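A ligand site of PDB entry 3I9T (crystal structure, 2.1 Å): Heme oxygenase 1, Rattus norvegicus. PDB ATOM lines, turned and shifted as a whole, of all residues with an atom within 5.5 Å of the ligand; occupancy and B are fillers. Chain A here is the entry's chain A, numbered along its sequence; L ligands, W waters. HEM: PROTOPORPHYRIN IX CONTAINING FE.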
ATOM      1  N   SER A  14       4.383  23.790   8.924  1.00  0.00           N
ATOM      2  CA  SER A  14       3.526  22.710   9.488  1.00  0.00           C
ATOM      3  C   SER A  14       2.001  22.964   9.343  1.00  0.00           C
ATOM      4  O   SER A  14       1.232  22.017   9.067  1.00  0.00           O
ATOM      5  CB  SER A  14       3.859  22.487  10.979  1.00  0.00           C
ATOM      6  OG  SER A  14       3.698  23.738  11.661  1.00  0.00           O
ATOM      7  N   LEU A  17       1.014  22.789   5.511  1.00  0.00           N
ATOM      8  CA  LEU A  17       0.860  21.389   5.126  1.00  0.00           C
ATOM      9  C   LEU A  17      -0.498  20.747   5.626  1.00  0.00           C
ATOM     10  O   LEU A  17      -1.154  19.976   4.870  1.00  0.00           O
ATOM     11  CB  LEU A  17       2.063  20.548   5.619  1.00  0.00           C
ATOM     12  CG  LEU A  17       3.334  20.661   4.750  1.00  0.00           C
ATOM     13  CD1 LEU A  17       4.659  20.035   5.400  1.00  0.00           C
ATOM     14  CD2 LEU A  17       3.058  19.928   3.472  1.00  0.00           C
ATOM     15  N   LYS A  18      -0.860  20.992   6.894  1.00  0.00           N
ATOM     16  CA  LYS A  18      -2.099  20.463   7.449  1.00  0.00           C
ATOM     17  C   LYS A  18      -3.267  21.024   6.599  1.00  0.00           C
ATOM     18  O   LYS A  18      -4.112  20.270   6.127  1.00  0.00           O
ATOM     19  CB  LYS A  18      -2.269  20.855   8.951  1.00  0.00           C
ATOM     20  CG  LYS A  18      -3.465  20.115   9.752  1.00  0.00           C
ATOM     21  CD  LYS A  18      -3.673  20.873  11.143  1.00  0.00           C
ATOM     22  CE  LYS A  18      -4.773  20.285  12.105  1.00  0.00           C
ATOM     23  NZ  LYS A  18      -4.646  18.808  12.293  1.00  0.00           N
ATOM     24  N   HIS A  25      -6.884  14.308   2.741  1.00  0.00           N
ATOM     25  CA  HIS A  25      -6.850  13.314   3.843  1.00  0.00           C
ATOM     26  C   HIS A  25      -8.290  12.710   4.014  1.00  0.00           C
ATOM     27  O   HIS A  25      -8.474  11.476   4.143  1.00  0.00           O
ATOM     28  CB  HIS A  25      -6.387  13.998   5.144  1.00  0.00           C
ATOM     29  CG  HIS A  25      -6.298  13.049   6.290  1.00  0.00           C
ATOM     30  ND1 HIS A  25      -7.421  12.453   6.851  1.00  0.00           N
ATOM     31  CD2 HIS A  25      -5.229  12.498   6.909  1.00  0.00           C
ATOM     32  CE1 HIS A  25      -7.037  11.596   7.786  1.00  0.00           C
ATOM     33  NE2 HIS A  25      -5.720  11.630   7.860  1.00  0.00           N
ATOM     34  N   ALA A  28      -8.594  10.098   1.389  1.00  0.00           N
ATOM     35  CA  ALA A  28      -7.795   8.925   1.718  1.00  0.00           C
ATOM     36  C   ALA A  28      -8.428   8.041   2.811  1.00  0.00           C
ATOM     37  O   ALA A  28      -8.431   6.867   2.685  1.00  0.00           O
ATOM     38  CB  ALA A  28      -6.327   9.313   2.085  1.00  0.00           C
ATOM     39  N   GLU A  29      -8.938   8.645   3.845  1.00  0.00           N
ATOM     40  CA  GLU A  29      -9.688   7.970   4.876  1.00  0.00           C
ATOM     41  C   GLU A  29     -10.808   7.098   4.315  1.00  0.00           C
ATOM     42  O   GLU A  29     -11.079   6.007   4.917  1.00  0.00           O
ATOM     43  CB  GLU A  29     -10.376   9.026   5.704  1.00  0.00           C
ATOM     44  CG  GLU A  29      -9.595   9.392   6.802  1.00  0.00           C
ATOM     45  CD  GLU A  29     -10.311  10.372   7.636  1.00  0.00           C
ATOM     46  OE1 GLU A  29     -10.384  11.589   7.280  1.00  0.00           O
ATOM     47  OE2 GLU A  29     -10.734   9.933   8.714  1.00  0.00           O
ATOM     48  N   ASN A  30     -11.444   7.543   3.205  1.00  0.00           N
ATOM     49  CA  ASN A  30     -12.534   6.824   2.632  1.00  0.00           C
ATOM     50  C   ASN A  30     -12.252   6.037   1.383  1.00  0.00           C
ATOM     51  O   ASN A  30     -13.202   5.620   0.702  1.00  0.00           O
ATOM     52  CB  ASN A  30     -13.717   7.730   2.397  1.00  0.00           C
ATOM     53  CG  ASN A  30     -14.255   8.291   3.655  1.00  0.00           C
ATOM     54  OD1 ASN A  30     -15.300   7.833   4.134  1.00  0.00           O
ATOM     55  ND2 ASN A  30     -13.605   9.304   4.201  1.00  0.00           N
ATOM     56  N   MET A  34      -9.316   1.577   3.159  1.00  0.00           N
ATOM     57  CA  MET A  34      -9.214   2.192   4.502  1.00  0.00           C
ATOM     58  C   MET A  34     -10.532   2.172   5.242  1.00  0.00           C
ATOM     59  O   MET A  34     -10.570   1.961   6.443  1.00  0.00           O
ATOM     60  CB  MET A  34      -8.599   3.619   4.480  1.00  0.00           C
ATOM     61  CG  MET A  34      -7.183   3.620   4.008  1.00  0.00           C
ATOM     62  SD  MET A  34      -6.328   2.746   5.354  1.00  0.00           S
ATOM     63  CE  MET A  34      -5.045   1.916   4.476  1.00  0.00           C
ATOM     64  N   ARG A  35     -11.631   2.311   4.492  1.00  0.00           N
ATOM     65  CA  ARG A  35     -12.999   2.240   5.055  1.00  0.00           C
ATOM     66  C   ARG A  35     -13.239   0.811   5.670  1.00  0.00           C
ATOM     67  O   ARG A  35     -13.588   0.697   6.850  1.00  0.00           O
ATOM     68  CB  ARG A  35     -13.980   2.512   3.924  1.00  0.00           C
ATOM     69  CG  ARG A  35     -15.187   3.364   4.271  1.00  0.00           C
ATOM     70  CD  ARG A  35     -15.837   3.872   3.000  1.00  0.00           C
ATOM     71  NE  ARG A  35     -16.250   2.814   2.061  1.00  0.00           N
ATOM     72  CZ  ARG A  35     -16.290   2.940   0.724  1.00  0.00           C
ATOM     73  NH1 ARG A  35     -15.892   4.084   0.075  1.00  0.00           N
ATOM     74  NH2 ARG A  35     -16.696   1.901   0.009  1.00  0.00           N
ATOM     75  N   GLN A  38     -10.830   0.248   8.793  1.00  0.00           N
ATOM     76  CA  GLN A  38     -11.364   0.949   9.937  1.00  0.00           C
ATOM     77  C   GLN A  38     -12.517   0.309  10.616  1.00  0.00           C
ATOM     78  O   GLN A  38     -12.666   0.517  11.817  1.00  0.00           O
ATOM     79  CB  GLN A  38     -11.881   2.305   9.524  1.00  0.00           C
ATOM     80  CG  GLN A  38     -10.929   3.355   9.685  1.00  0.00           C
ATOM     81  CD  GLN A  38     -11.600   4.680   9.831  1.00  0.00           C
ATOM     82  OE1 GLN A  38     -11.621   5.270  10.925  1.00  0.00           O
ATOM     83  NE2 GLN A  38     -12.146   5.202   8.712  1.00  0.00           N
ATOM     84  N   TYR A 114       4.974   4.828  -6.538  1.00  0.00           N
ATOM     85  CA  TYR A 114       5.320   5.592  -5.349  1.00  0.00           C
ATOM     86  C   TYR A 114       6.862   5.608  -5.070  1.00  0.00           C
ATOM     87  O   TYR A 114       7.471   6.674  -4.916  1.00  0.00           O
ATOM     88  CB  TYR A 114       4.549   4.962  -4.178  1.00  0.00           C
ATOM     89  CG  TYR A 114       4.345   5.801  -2.921  1.00  0.00           C
ATOM     90  CD1 TYR A 114       5.184   6.865  -2.588  1.00  0.00           C
ATOM     91  CD2 TYR A 114       3.363   5.426  -1.995  1.00  0.00           C
ATOM     92  CE1 TYR A 114       5.026   7.542  -1.379  1.00  0.00           C
ATOM     93  CE2 TYR A 114       3.177   6.120  -0.834  1.00  0.00           C
ATOM     94  CZ  TYR A 114       4.008   7.148  -0.507  1.00  0.00           C
ATOM     95  OH  TYR A 114       3.786   7.807   0.689  1.00  0.00           O
ATOM     96  N   TYR A 134       6.702  14.043   5.992  1.00  0.00           N
ATOM     97  CA  TYR A 134       5.496  14.522   6.684  1.00  0.00           C
ATOM     98  C   TYR A 134       4.298  13.585   6.457  1.00  0.00           C
ATOM     99  O   TYR A 134       3.613  13.171   7.442  1.00  0.00           O
ATOM    100  CB  TYR A 134       5.141  15.966   6.188  1.00  0.00           C
ATOM    101  CG  TYR A 134       3.726  16.371   6.491  1.00  0.00           C
ATOM    102  CD1 TYR A 134       3.396  16.916   7.725  1.00  0.00           C
ATOM    103  CD2 TYR A 134       2.704  16.253   5.518  1.00  0.00           C
ATOM    104  CE1 TYR A 134       2.115  17.303   8.043  1.00  0.00           C
ATOM    105  CE2 TYR A 134       1.343  16.614   5.848  1.00  0.00           C
ATOM    106  CZ  TYR A 134       1.076  17.165   7.114  1.00  0.00           C
ATOM    107  OH  TYR A 134      -0.207  17.557   7.507  1.00  0.00           O
ATOM    108  N   THR A 135       4.021  13.220   5.195  1.00  0.00           N
ATOM    109  CA  THR A 135       2.793  12.503   4.884  1.00  0.00           C
ATOM    110  C   THR A 135       2.753  11.129   5.560  1.00  0.00           C
ATOM    111  O   THR A 135       1.711  10.666   6.052  1.00  0.00           O
ATOM    112  CB  THR A 135       2.640  12.348   3.324  1.00  0.00           C
ATOM    113  OG1 THR A 135       2.465  13.661   2.777  1.00  0.00           O
ATOM    114  CG2 THR A 135       1.466  11.410   2.863  1.00  0.00           C
ATOM    115  N   ARG A 136       3.901  10.474   5.573  1.00  0.00           N
ATOM    116  CA  ARG A 136       4.038   9.144   6.124  1.00  0.00           C
ATOM    117  C   ARG A 136       4.200   9.225   7.672  1.00  0.00           C
ATOM    118  O   ARG A 136       3.318   8.836   8.374  1.00  0.00           O
ATOM    119  CB  ARG A 136       5.235   8.425   5.502  1.00  0.00           C
ATOM    120  CG  ARG A 136       4.923   7.780   4.026  1.00  0.00           C
ATOM    121  CD  ARG A 136       3.639   6.826   3.874  1.00  0.00           C
ATOM    122  NE  ARG A 136       3.284   6.114   5.089  1.00  0.00           N
ATOM    123  CZ  ARG A 136       2.170   5.397   5.277  1.00  0.00           C
ATOM    124  NH1 ARG A 136       1.286   5.305   4.313  1.00  0.00           N
ATOM    125  NH2 ARG A 136       1.884   4.818   6.458  1.00  0.00           N
ATOM    126  N   LEU A 138       4.135  11.619  10.149  1.00  0.00           N
ATOM    127  CA  LEU A 138       3.096  12.263  10.987  1.00  0.00           C
ATOM    128  C   LEU A 138       1.758  11.537  11.078  1.00  0.00           C
ATOM    129  O   LEU A 138       1.073  11.585  12.130  1.00  0.00           O
ATOM    130  CB  LEU A 138       2.889  13.719  10.612  1.00  0.00           C
ATOM    131  CG  LEU A 138       3.813  14.842  11.196  1.00  0.00           C
ATOM    132  CD1 LEU A 138       3.019  15.990  11.711  1.00  0.00           C
ATOM    133  CD2 LEU A 138       4.802  14.418  12.278  1.00  0.00           C
ATOM    134  N   GLY A 139       1.323  10.901   9.967  1.00  0.00           N
ATOM    135  CA  GLY A 139       0.173  10.046  10.030  1.00  0.00           C
ATOM    136  C   GLY A 139       0.514   8.849  10.870  1.00  0.00           C
ATOM    137  O   GLY A 139      -0.328   8.429  11.675  1.00  0.00           O
ATOM    138  N   SER A 142      -0.236   9.477  14.221  1.00  0.00           N
ATOM    139  CA  SER A 142      -1.618   9.926  14.510  1.00  0.00           C
ATOM    140  C   SER A 142      -2.629   8.790  14.311  1.00  0.00           C
ATOM    141  O   SER A 142      -2.798   7.888  15.138  1.00  0.00           O
ATOM    142  CB  SER A 142      -1.934  11.064  13.578  1.00  0.00           C
ATOM    143  OG  SER A 142      -0.965  12.026  13.735  1.00  0.00           O
ATOM    144  N   GLY A 143      -3.270   8.791  13.161  1.00  0.00           N
ATOM    145  CA  GLY A 143      -4.264   7.767  12.863  1.00  0.00           C
ATOM    146  C   GLY A 143      -3.663   6.367  12.841  1.00  0.00           C
ATOM    147  O   GLY A 143      -4.341   5.411  13.187  1.00  0.00           O
ATOM    148  N   VAL A 146      -4.395   4.489  15.870  1.00  0.00           N
ATOM    149  CA  VAL A 146      -5.767   3.980  15.902  1.00  0.00           C
ATOM    150  C   VAL A 146      -5.839   2.748  15.010  1.00  0.00           C
ATOM    151  O   VAL A 146      -6.375   1.743  15.452  1.00  0.00           O
ATOM    152  CB  VAL A 146      -6.790   5.070  15.459  1.00  0.00           C
ATOM    153  CG1 VAL A 146      -8.239   4.529  15.516  1.00  0.00           C
ATOM    154  CG2 VAL A 146      -6.610   6.360  16.367  1.00  0.00           C
ATOM    155  N   LEU A 147      -5.271   2.800  13.791  1.00  0.00           N
ATOM    156  CA  LEU A 147      -5.325   1.623  12.943  1.00  0.00           C
ATOM    157  C   LEU A 147      -4.655   0.393  13.577  1.00  0.00           C
ATOM    158  O   LEU A 147      -5.148  -0.701  13.446  1.00  0.00           O
ATOM    159  CB  LEU A 147      -4.729   1.882  11.535  1.00  0.00           C
ATOM    160  CG  LEU A 147      -5.510   3.003  10.780  1.00  0.00           C
ATOM    161  CD1 LEU A 147      -4.815   3.304   9.473  1.00  0.00           C
ATOM    162  CD2 LEU A 147      -6.991   2.624  10.558  1.00  0.00           C
ATOM    163  N   ARG A 183       6.927  19.282  14.173  1.00  0.00           N
ATOM    164  CA  ARG A 183       6.330  20.482  13.576  1.00  0.00           C
ATOM    165  C   ARG A 183       7.143  21.743  13.764  1.00  0.00           C
ATOM    166  O   ARG A 183       7.353  22.506  12.804  1.00  0.00           O
ATOM    167  CB  ARG A 183       4.895  20.716  14.073  1.00  0.00           C
ATOM    168  CG  ARG A 183       3.865  19.671  13.558  1.00  0.00           C
ATOM    169  CD  ARG A 183       2.442  20.208  13.835  1.00  0.00           C
ATOM    170  NE  ARG A 183       1.489  19.147  13.693  1.00  0.00           N
ATOM    171  CZ  ARG A 183       1.046  18.388  14.679  1.00  0.00           C
ATOM    172  NH1 ARG A 183       1.461  18.605  15.951  1.00  0.00           N
ATOM    173  NH2 ARG A 183       0.183  17.405  14.399  1.00  0.00           N
ATOM    174  N   ALA A 206       1.769  12.980  -2.575  1.00  0.00           N
ATOM    175  CA  ALA A 206       2.146  11.833  -1.755  1.00  0.00           C
ATOM    176  C   ALA A 206       0.846  11.199  -1.270  1.00  0.00           C
ATOM    177  O   ALA A 206       0.733   9.995  -1.230  1.00  0.00           O
ATOM    178  CB  ALA A 206       3.020  12.345  -0.490  1.00  0.00           C
ATOM    179  N   PHE A 207      -0.131  12.008  -0.926  1.00  0.00           N
ATOM    180  CA  PHE A 207      -1.453  11.463  -0.482  1.00  0.00           C
ATOM    181  C   PHE A 207      -2.135  10.766  -1.616  1.00  0.00           C
ATOM    182  O   PHE A 207      -2.685   9.682  -1.425  1.00  0.00           O
ATOM    183  CB  PHE A 207      -2.366  12.573  -0.004  1.00  0.00           C
ATOM    184  CG  PHE A 207      -2.337  12.788   1.453  1.00  0.00           C
ATOM    185  CD1 PHE A 207      -1.376  13.654   2.020  1.00  0.00           C
ATOM    186  CD2 PHE A 207      -3.264  12.150   2.281  1.00  0.00           C
ATOM    187  CE1 PHE A 207      -1.347  13.885   3.387  1.00  0.00           C
ATOM    188  CE2 PHE A 207      -3.264  12.380   3.672  1.00  0.00           C
ATOM    189  CZ  PHE A 207      -2.291  13.237   4.240  1.00  0.00           C
ATOM    190  N   ASN A 210      -0.682   7.356  -2.122  1.00  0.00           N
ATOM    191  CA  ASN A 210      -1.236   6.464  -1.130  1.00  0.00           C
ATOM    192  C   ASN A 210      -2.632   5.990  -1.552  1.00  0.00           C
ATOM    193  O   ASN A 210      -2.917   4.785  -1.523  1.00  0.00           O
ATOM    194  CB  ASN A 210      -1.257   7.118   0.252  1.00  0.00           C
ATOM    195  CG  ASN A 210       0.119   7.010   0.947  1.00  0.00           C
ATOM    196  OD1 ASN A 210       0.471   5.951   1.515  1.00  0.00           O
ATOM    197  ND2 ASN A 210       0.953   8.031   0.743  1.00  0.00           N
ATOM    198  N   PHE A 214      -4.032   2.148  -2.363  1.00  0.00           N
ATOM    199  CA  PHE A 214      -5.187   1.498  -1.752  1.00  0.00           C
ATOM    200  C   PHE A 214      -6.183   1.016  -2.795  1.00  0.00           C
ATOM    201  O   PHE A 214      -6.673  -0.113  -2.676  1.00  0.00           O
ATOM    202  CB  PHE A 214      -5.851   2.430  -0.778  1.00  0.00           C
ATOM    203  CG  PHE A 214      -4.930   2.884   0.325  1.00  0.00           C
ATOM    204  CD1 PHE A 214      -3.962   1.981   0.830  1.00  0.00           C
ATOM    205  CD2 PHE A 214      -5.025   4.166   0.870  1.00  0.00           C
ATOM    206  CE1 PHE A 214      -3.041   2.374   1.807  1.00  0.00           C
ATOM    207  CE2 PHE A 214      -4.121   4.550   1.872  1.00  0.00           C
ATOM    208  CZ  PHE A 214      -3.139   3.625   2.339  1.00  0.00           C
HETATM  209  CHA HEM L   1      -3.569  12.918  11.008  1.00  0.00           C
HETATM  210  CHB HEM L   1      -6.812   9.303  11.167  1.00  0.00           C
HETATM  211  CHC HEM L   1      -5.577   7.841   6.659  1.00  0.00           C
HETATM  212  CHD HEM L   1      -1.839  10.917   6.899  1.00  0.00           C
HETATM  213  C1A HEM L   1      -4.618  12.101  11.389  1.00  0.00           C
HETATM  214  C2A HEM L   1      -5.399  12.261  12.603  1.00  0.00           C
HETATM  215  C3A HEM L   1      -6.267  11.265  12.658  1.00  0.00           C
HETATM  216  C4A HEM L   1      -6.097  10.447  11.469  1.00  0.00           C
HETATM  217  CMA HEM L   1      -7.350  11.085  13.769  1.00  0.00           C
HETATM  218  CAA HEM L   1      -5.227  13.438  13.615  1.00  0.00           C
HETATM  219  CBA HEM L   1      -6.013  14.634  13.066  1.00  0.00           C
HETATM  220  CGA HEM L   1      -6.004  15.786  14.053  1.00  0.00           C
HETATM  221  O1A HEM L   1      -6.006  15.543  15.309  1.00  0.00           O
HETATM  222  O2A HEM L   1      -6.032  16.944  13.575  1.00  0.00           O
HETATM  223  C1B HEM L   1      -6.742   8.541  10.003  1.00  0.00           C
HETATM  224  C2B HEM L   1      -7.485   7.309   9.709  1.00  0.00           C
HETATM  225  C3B HEM L   1      -7.162   6.961   8.446  1.00  0.00           C
HETATM  226  C4B HEM L   1      -6.162   7.903   7.920  1.00  0.00           C
HETATM  227  CMB HEM L   1      -8.501   6.617  10.653  1.00  0.00           C
HETATM  228  CAB HEM L   1      -7.640   5.750   7.642  1.00  0.00           C
HETATM  229  CBB HEM L   1      -8.940   5.543   7.580  1.00  0.00           C
HETATM  230  C1C HEM L   1      -4.428   8.495   6.310  1.00  0.00           C
HETATM  231  C2C HEM L   1      -3.644   8.327   5.091  1.00  0.00           C
HETATM  232  C3C HEM L   1      -2.590   9.196   5.211  1.00  0.00           C
HETATM  233  C4C HEM L   1      -2.715   9.959   6.441  1.00  0.00           C
HETATM  234  CMC HEM L   1      -3.894   7.365   3.887  1.00  0.00           C
HETATM  235  CAC HEM L   1      -1.489   9.442   4.124  1.00  0.00           C
HETATM  236  CBC HEM L   1      -0.554   8.572   3.773  1.00  0.00           C
HETATM  237  C1D HEM L   1      -1.960  11.757   7.978  1.00  0.00           C
HETATM  238  C2D HEM L   1      -1.075  12.895   8.257  1.00  0.00           C
HETATM  239  C3D HEM L   1      -1.602  13.520   9.516  1.00  0.00           C
HETATM  240  C4D HEM L   1      -2.757  12.712   9.893  1.00  0.00           C
HETATM  241  CMD HEM L   1       0.122  13.350   7.422  1.00  0.00           C
HETATM  242  CAD HEM L   1      -1.006  14.734  10.268  1.00  0.00           C
HETATM  243  CBD HEM L   1      -1.902  15.945   9.996  1.00  0.00           C
HETATM  244  CGD HEM L   1      -1.218  17.106  10.688  1.00  0.00           C
HETATM  245  O1D HEM L   1      -0.712  18.034  10.002  1.00  0.00           O
HETATM  246  O2D HEM L   1      -1.127  17.071  11.945  1.00  0.00           O
HETATM  247  NA  HEM L   1      -5.063  10.986  10.716  1.00  0.00           N
HETATM  248  NB  HEM L   1      -5.986   8.873   8.893  1.00  0.00           N
HETATM  249  NC  HEM L   1      -3.819   9.498   7.098  1.00  0.00           N
HETATM  250  ND  HEM L   1      -2.957  11.734   8.940  1.00  0.00           N
HETATM  251 FE   HEM L   1      -4.426  10.317   8.893  1.00  0.00          FE
HETATM  252  O   HOH W   1      -6.311  14.377   9.734  1.00  0.00           O
HETATM  253  O   HOH W   2       0.933  19.756  10.903  1.00  0.00           O
HETATM  254  O   HOH W   3      -1.961  15.109  13.915  1.00  0.00           O
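Residues that only touch the ligand: Asn 210, Thr 135, Gln 38, Gly 139, Gly 143, Glu 29, Phe 207, Phe 214, Ser 142, Ala 28, Met 34 and Arg 136.
Hydrophobic or aromatic side chains that line the ligand: His 25, Ala 28, Met 34, Tyr 134, Phe 207 and Phe 214.
16 residues have an atom within 4 Å of the ligand: Lys 18, His 25, Ala 28, Glu 29, Met 34, Gln 38, Tyr 134, Thr 135, Arg 136, Gly 139, Ser 142, Gly 143, Arg 183, Phe 207, Asn 210 and Phe 214.
The backbone carbonyl oxygen of Leu 138 sits at hydrogen-bond distance from the side-chain hydroxyl of Ser 142, 2.6 Å away.
OD1 of Asn 210 sits at hydrogen-bond distance from NH1 of Arg 136 (3.0 Å).
ND2 of Asn 210 is in hydrogen-bond range of O of Ala 206.
ND1 of His 25 is in hydrogen-bond range of OE1 of Glu 29, 3.1 Å away.
The side-chain hydroxyl (OH) of Tyr 114 is in hydrogen-bond range of the side-chain amide nitrogen (ND2) of Asn 210, at 2.8 Å.
Water W2 lies within hydrogen-bond range of an oxygen (O1D) of the ligand (2.5 Å), the guanidinium group of Arg 183 (2.9 Å) and the backbone carbonyl oxygen of Ser 14 (2.9 Å).
Water W3 lies within hydrogen-bond range of O2D of the ligand, NH2 of Arg 183 and OG of Ser 142.
NE2 of His 25 binds FE of the ligand (2.1 Å).
An oxygen (O2A) of the ligand lies within salt-bridge range of the side-chain amino group (NZ) of Lys 18 (2.7 Å).
O2D of the ligand lies within salt-bridge range of NH2 of Arg 183.
O1D of the ligand lies within hydrogen-bond range of OH of Tyr 134 (2.6 Å).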
